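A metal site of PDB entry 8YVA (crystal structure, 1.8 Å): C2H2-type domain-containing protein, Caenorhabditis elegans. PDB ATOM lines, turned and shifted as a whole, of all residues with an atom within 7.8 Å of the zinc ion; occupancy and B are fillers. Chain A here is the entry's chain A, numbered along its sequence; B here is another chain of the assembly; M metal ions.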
ATOM      1  N   LYS A  27      10.207 -34.536 -21.140  1.00  0.00           N
ATOM      2  CA  LYS A  27      11.665 -34.601 -21.203  1.00  0.00           C
ATOM      3  C   LYS A  27      12.206 -33.675 -22.285  1.00  0.00           C
ATOM      4  O   LYS A  27      11.767 -33.761 -23.433  1.00  0.00           O
ATOM      5  CB  LYS A  27      12.131 -36.032 -21.478  1.00  0.00           C
ATOM      6  CG  LYS A  27      13.593 -36.226 -21.201  1.00  0.00           C
ATOM      7  CD  LYS A  27      14.140 -37.525 -21.780  1.00  0.00           C
ATOM      8  CE  LYS A  27      15.641 -37.636 -21.541  1.00  0.00           C
ATOM      9  NZ  LYS A  27      16.292 -38.582 -22.490  1.00  0.00           N
ATOM     10  N   CYS A  28      13.173 -32.829 -21.928  1.00  0.00           N
ATOM     11  CA  CYS A  28      13.824 -31.978 -22.926  1.00  0.00           C
ATOM     12  C   CYS A  28      14.993 -32.709 -23.578  1.00  0.00           C
ATOM     13  O   CYS A  28      15.991 -33.024 -22.909  1.00  0.00           O
ATOM     14  CB  CYS A  28      14.298 -30.667 -22.315  1.00  0.00           C
ATOM     15  SG  CYS A  28      15.143 -29.581 -23.536  1.00  0.00           S
ATOM     16  N   HIS A  29      14.919 -32.886 -24.894  1.00  0.00           N
ATOM     17  CA  HIS A  29      15.918 -33.575 -25.694  1.00  0.00           C
ATOM     18  C   HIS A  29      16.911 -32.651 -26.368  1.00  0.00           C
ATOM     19  O   HIS A  29      17.623 -33.078 -27.279  1.00  0.00           O
ATOM     20  CB  HIS A  29      15.215 -34.434 -26.740  1.00  0.00           C
ATOM     21  CG  HIS A  29      14.429 -35.557 -26.135  1.00  0.00           C
ATOM     22  ND1 HIS A  29      13.056 -35.581 -26.123  1.00  0.00           N
ATOM     23  CD2 HIS A  29      14.834 -36.674 -25.495  1.00  0.00           C
ATOM     24  CE1 HIS A  29      12.637 -36.683 -25.513  1.00  0.00           C
ATOM     25  NE2 HIS A  29      13.701 -37.355 -25.126  1.00  0.00           N
ATOM     26  N   PHE A  30      16.987 -31.383 -25.954  1.00  0.00           N
ATOM     27  CA  PHE A  30      18.061 -30.533 -26.444  1.00  0.00           C
ATOM     28  C   PHE A  30      19.403 -31.100 -25.984  1.00  0.00           C
ATOM     29  O   PHE A  30      19.505 -31.609 -24.863  1.00  0.00           O
ATOM     30  CB  PHE A  30      17.882 -29.108 -25.955  1.00  0.00           C
ATOM     31  CG  PHE A  30      18.584 -28.085 -26.789  1.00  0.00           C
ATOM     32  CD1 PHE A  30      17.966 -27.536 -27.915  1.00  0.00           C
ATOM     33  CD2 PHE A  30      19.846 -27.638 -26.445  1.00  0.00           C
ATOM     34  CE1 PHE A  30      18.613 -26.596 -28.678  1.00  0.00           C
ATOM     35  CE2 PHE A  30      20.488 -26.694 -27.195  1.00  0.00           C
ATOM     36  CZ  PHE A  30      19.871 -26.164 -28.315  1.00  0.00           C
ATOM     37  N   ASP A  31      20.408 -31.033 -26.857  1.00  0.00           N
ATOM     38  CA  ASP A  31      21.714 -31.632 -26.617  1.00  0.00           C
ATOM     39  C   ASP A  31      22.188 -31.409 -25.190  1.00  0.00           C
ATOM     40  O   ASP A  31      22.338 -30.258 -24.752  1.00  0.00           O
ATOM     41  CB  ASP A  31      22.751 -31.072 -27.594  1.00  0.00           C
ATOM     42  CG  ASP A  31      22.746 -31.792 -28.929  1.00  0.00           C
ATOM     43  OD1 ASP A  31      21.882 -32.662 -29.143  1.00  0.00           O
ATOM     44  OD2 ASP A  31      23.624 -31.484 -29.768  1.00  0.00           O
ATOM     45  N   ASN A  32      22.420 -32.514 -24.471  1.00  0.00           N
ATOM     46  CA  ASN A  32      22.923 -32.530 -23.097  1.00  0.00           C
ATOM     47  C   ASN A  32      22.077 -31.693 -22.146  1.00  0.00           C
ATOM     48  O   ASN A  32      22.573 -31.141 -21.155  1.00  0.00           O
ATOM     49  CB  ASN A  32      24.400 -32.147 -23.051  1.00  0.00           C
ATOM     50  CG  ASN A  32      25.190 -32.776 -24.198  1.00  0.00           C
ATOM     51  OD1 ASN A  32      24.832 -33.845 -24.693  1.00  0.00           O
ATOM     52  ND2 ASN A  32      26.254 -32.108 -24.631  1.00  0.00           N
ATOM     53  N   CYS A  33      20.782 -31.610 -22.417  1.00  0.00           N
ATOM     54  CA  CYS A  33      19.848 -31.142 -21.398  1.00  0.00           C
ATOM     55  C   CYS A  33      19.272 -32.336 -20.645  1.00  0.00           C
ATOM     56  O   CYS A  33      19.671 -32.616 -19.516  1.00  0.00           O
ATOM     57  CB  CYS A  33      18.741 -30.287 -21.991  1.00  0.00           C
ATOM     58  SG  CYS A  33      17.748 -29.597 -20.682  1.00  0.00           S
ATOM     59  N   ASN A  34      18.325 -33.051 -21.273  1.00  0.00           N
ATOM     60  CA  ASN A  34      17.678 -34.230 -20.689  1.00  0.00           C
ATOM     61  C   ASN A  34      16.986 -33.938 -19.361  1.00  0.00           C
ATOM     62  O   ASN A  34      16.688 -34.862 -18.604  1.00  0.00           O
ATOM     63  CB  ASN A  34      18.659 -35.397 -20.551  1.00  0.00           C
ATOM     64  CG  ASN A  34      19.241 -35.818 -21.882  1.00  0.00           C
ATOM     65  OD1 ASN A  34      18.501 -36.108 -22.829  1.00  0.00           O
ATOM     66  ND2 ASN A  34      20.560 -35.859 -21.960  1.00  0.00           N
ATOM     67  N   ARG A  35      16.706 -32.667 -19.074  1.00  0.00           N
ATOM     68  CA  ARG A  35      15.893 -32.318 -17.913  1.00  0.00           C
ATOM     69  C   ARG A  35      14.455 -32.789 -18.129  1.00  0.00           C
ATOM     70  O   ARG A  35      13.981 -32.924 -19.264  1.00  0.00           O
ATOM     71  CB  ARG A  35      15.921 -30.805 -17.712  1.00  0.00           C
ATOM     72  CG  ARG A  35      17.328 -30.255 -17.447  1.00  0.00           C
ATOM     73  CD  ARG A  35      17.889 -30.537 -16.084  1.00  0.00           C
ATOM     74  NE  ARG A  35      16.969 -30.096 -15.052  1.00  0.00           N
ATOM     75  CZ  ARG A  35      17.199 -30.175 -13.756  1.00  0.00           C
ATOM     76  NH1 ARG A  35      18.351 -30.625 -13.280  1.00  0.00           N
ATOM     77  NH2 ARG A  35      16.254 -29.781 -12.896  1.00  0.00           N
ATOM     78  N   LYS A  36      13.761 -33.047 -17.027  1.00  0.00           N
ATOM     79  CA  LYS A  36      12.370 -33.442 -17.080  1.00  0.00           C
ATOM     80  C   LYS A  36      11.542 -32.364 -16.389  1.00  0.00           C
ATOM     81  O   LYS A  36      11.790 -32.041 -15.218  1.00  0.00           O
ATOM     82  CB  LYS A  36      12.175 -34.806 -16.418  1.00  0.00           C
ATOM     83  CG  LYS A  36      12.526 -35.991 -17.334  1.00  0.00           C
ATOM     84  CD  LYS A  36      13.069 -37.194 -16.549  1.00  0.00           C
ATOM     85  CE  LYS A  36      14.437 -36.891 -15.951  1.00  0.00           C
ATOM     86  NZ  LYS A  36      14.835 -37.866 -14.915  1.00  0.00           N
ATOM     87  N   ILE A  37      10.580 -31.800 -17.104  1.00  0.00           N
ATOM     88  CA  ILE A  37       9.648 -30.843 -16.517  1.00  0.00           C
ATOM     89  C   ILE A  37       8.448 -31.599 -15.990  1.00  0.00           C
ATOM     90  O   ILE A  37       7.808 -32.357 -16.736  1.00  0.00           O
ATOM     91  CB  ILE A  37       9.232 -29.783 -17.548  1.00  0.00           C
ATOM     92  CG1 ILE A  37      10.489 -29.153 -18.171  1.00  0.00           C
ATOM     93  CG2 ILE A  37       8.269 -28.766 -16.906  1.00  0.00           C
ATOM     94  CD1 ILE A  37      11.271 -28.310 -17.211  1.00  0.00           C
ATOM     95  N   HIS A  51      11.225 -22.897 -21.367  1.00  0.00           N
ATOM     96  CA  HIS A  51      12.375 -23.797 -21.354  1.00  0.00           C
ATOM     97  C   HIS A  51      12.995 -23.881 -22.751  1.00  0.00           C
ATOM     98  O   HIS A  51      14.225 -23.792 -22.909  1.00  0.00           O
ATOM     99  CB  HIS A  51      11.971 -25.172 -20.836  1.00  0.00           C
ATOM    100  CG  HIS A  51      13.137 -26.077 -20.652  1.00  0.00           C
ATOM    101  ND1 HIS A  51      13.873 -26.104 -19.485  1.00  0.00           N
ATOM    102  CD2 HIS A  51      13.757 -26.930 -21.509  1.00  0.00           C
ATOM    103  CE1 HIS A  51      14.879 -26.949 -19.615  1.00  0.00           C
ATOM    104  NE2 HIS A  51      14.825 -27.474 -20.835  1.00  0.00           N
ATOM    105  N   ALA A  52      12.162 -24.044 -23.786  1.00  0.00           N
ATOM    106  CA  ALA A  52      12.683 -24.057 -25.153  1.00  0.00           C
ATOM    107  C   ALA A  52      13.328 -22.720 -25.516  1.00  0.00           C
ATOM    108  O   ALA A  52      14.397 -22.691 -26.161  1.00  0.00           O
ATOM    109  CB  ALA A  52      11.563 -24.420 -26.141  1.00  0.00           C
ATOM    110  N   SER A  54      14.889 -20.820 -23.620  1.00  0.00           N
ATOM    111  CA  SER A  54      16.177 -20.735 -22.939  1.00  0.00           C
ATOM    112  C   SER A  54      17.289 -21.434 -23.714  1.00  0.00           C
ATOM    113  O   SER A  54      18.468 -21.189 -23.433  1.00  0.00           O
ATOM    114  CB  SER A  54      16.081 -21.298 -21.523  1.00  0.00           C
ATOM    115  OG  SER A  54      16.016 -22.727 -21.507  1.00  0.00           O
ATOM    116  N   HIS A  55      16.950 -22.295 -24.661  1.00  0.00           N
ATOM    117  CA  HIS A  55      17.941 -22.999 -25.474  1.00  0.00           C
ATOM    118  C   HIS A  55      18.248 -22.265 -26.767  1.00  0.00           C
ATOM    119  O   HIS A  55      19.048 -22.759 -27.572  1.00  0.00           O
ATOM    120  CB  HIS A  55      17.425 -24.397 -25.805  1.00  0.00           C
ATOM    121  CG  HIS A  55      17.530 -25.352 -24.663  1.00  0.00           C
ATOM    122  ND1 HIS A  55      18.697 -25.556 -23.958  1.00  0.00           N
ATOM    123  CD2 HIS A  55      16.605 -26.161 -24.090  1.00  0.00           C
ATOM    124  CE1 HIS A  55      18.497 -26.448 -23.015  1.00  0.00           C
ATOM    125  NE2 HIS A  55      17.235 -26.844 -23.079  1.00  0.00           N
ATOM    126  N   CYS A 111      13.413 -29.811 -28.538  1.00  0.00           N
ATOM    127  CA  CYS A 111      13.259 -30.089 -27.118  1.00  0.00           C
ATOM    128  C   CYS A 111      12.201 -31.157 -26.871  1.00  0.00           C
ATOM    129  O   CYS A 111      12.457 -32.137 -26.161  1.00  0.00           O
ATOM    130  CB  CYS A 111      12.872 -28.804 -26.371  1.00  0.00           C
ATOM    131  SG  CYS A 111      14.175 -27.579 -26.354  1.00  0.00           S
ATOM    132  N   PHE A 112      11.010 -30.979 -27.434  1.00  0.00           N
ATOM    133  CA  PHE A 112       9.839 -31.720 -26.989  1.00  0.00           C
ATOM    134  C   PHE A 112       9.073 -32.389 -28.125  1.00  0.00           C
ATOM    135  O   PHE A 112       7.972 -32.900 -27.880  1.00  0.00           O
ATOM    136  CB  PHE A 112       8.876 -30.801 -26.229  1.00  0.00           C
ATOM    137  CG  PHE A 112       9.506 -30.022 -25.103  1.00  0.00           C
ATOM    138  CD1 PHE A 112      10.190 -30.670 -24.087  1.00  0.00           C
ATOM    139  CD2 PHE A 112       9.412 -28.640 -25.064  1.00  0.00           C
ATOM    140  CE1 PHE A 112      10.774 -29.939 -23.039  1.00  0.00           C
ATOM    141  CE2 PHE A 112       9.992 -27.921 -24.021  1.00  0.00           C
ATOM    142  CZ  PHE A 112      10.670 -28.563 -23.016  1.00  0.00           C
ATOM    143  P    DG B   5      14.027 -25.291 -16.048  1.00  0.00           P
ATOM    144  OP1  DG B   5      14.783 -26.543 -16.245  1.00  0.00           O
ATOM    145  OP2  DG B   5      13.276 -24.672 -17.148  1.00  0.00           O
ATOM    146  O5'  DG B   5      12.945 -25.520 -14.898  1.00  0.00           O
ATOM    147  C5'  DG B   5      13.319 -26.076 -13.647  1.00  0.00           C
ATOM    148  C4'  DG B   5      12.161 -25.957 -12.683  1.00  0.00           C
ATOM    149  O4'  DG B   5      12.136 -24.614 -12.131  1.00  0.00           O
ATOM    150  C3'  DG B   5      10.760 -26.183 -13.301  1.00  0.00           C
ATOM    151  O3'  DG B   5       9.921 -26.937 -12.413  1.00  0.00           O
ATOM    152  C2'  DG B   5      10.232 -24.767 -13.417  1.00  0.00           C
ATOM    153  C1'  DG B   5      10.797 -24.210 -12.132  1.00  0.00           C
ATOM    154  N9   DG B   5      10.686 -22.761 -11.987  1.00  0.00           N
ATOM    155  C8   DG B   5      10.590 -21.817 -12.975  1.00  0.00           C
ATOM    156  N7   DG B   5      10.449 -20.608 -12.504  1.00  0.00           N
ATOM    157  C5   DG B   5      10.404 -20.780 -11.121  1.00  0.00           C
ATOM    158  C6   DG B   5      10.251 -19.834 -10.076  1.00  0.00           C
ATOM    159  O6   DG B   5      10.116 -18.601 -10.165  1.00  0.00           O
ATOM    160  N1   DG B   5      10.264 -20.435  -8.814  1.00  0.00           N
ATOM    161  C2   DG B   5      10.422 -21.794  -8.599  1.00  0.00           C
ATOM    162  N2   DG B   5      10.400 -22.212  -7.322  1.00  0.00           N
ATOM    163  N3   DG B   5      10.566 -22.682  -9.563  1.00  0.00           N
ATOM    164  C4   DG B   5      10.541 -22.104 -10.798  1.00  0.00           C
HETATM  165 ZN    ZN M   1      16.312 -28.402 -22.035  1.00  0.00          ZN
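The zinc ion is bound by NE2 of His 55 (2.1 Å), NE2 of His 51 (2.1 Å), SG of Cys 28 (2.2 Å) and SG of Cys 33 (2.3 Å).
The zinc ion has four donor atoms within binding distance.
The backbone NH (N) of Arg 35 sits close to the side-chain sulfur (SG) of Cys 33 (3.6 Å).
N of Cys 28 is in hydrogen-bond range of O of Arg 35 (2.8 Å).
N of Asn 34 is in hydrogen-bond range of O of Cys 28.
The side-chain hydroxyl (OG) of Ser 54 sits at hydrogen-bond distance from the backbone carbonyl oxygen (O) of His 51 (2.5 Å).
N of Phe 30 sits close to SG of Cys 28, at 3.5 Å.
The side-chain sulfur (SG) of Cys 111 lies close to the side-chain sulfur (SG) of Cys 28, 3.6 Å away.
A ring nitrogen (ND1) of His 51 is in hydrogen-bond range of OP2 of DG 5 of chain B (2.8 Å).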
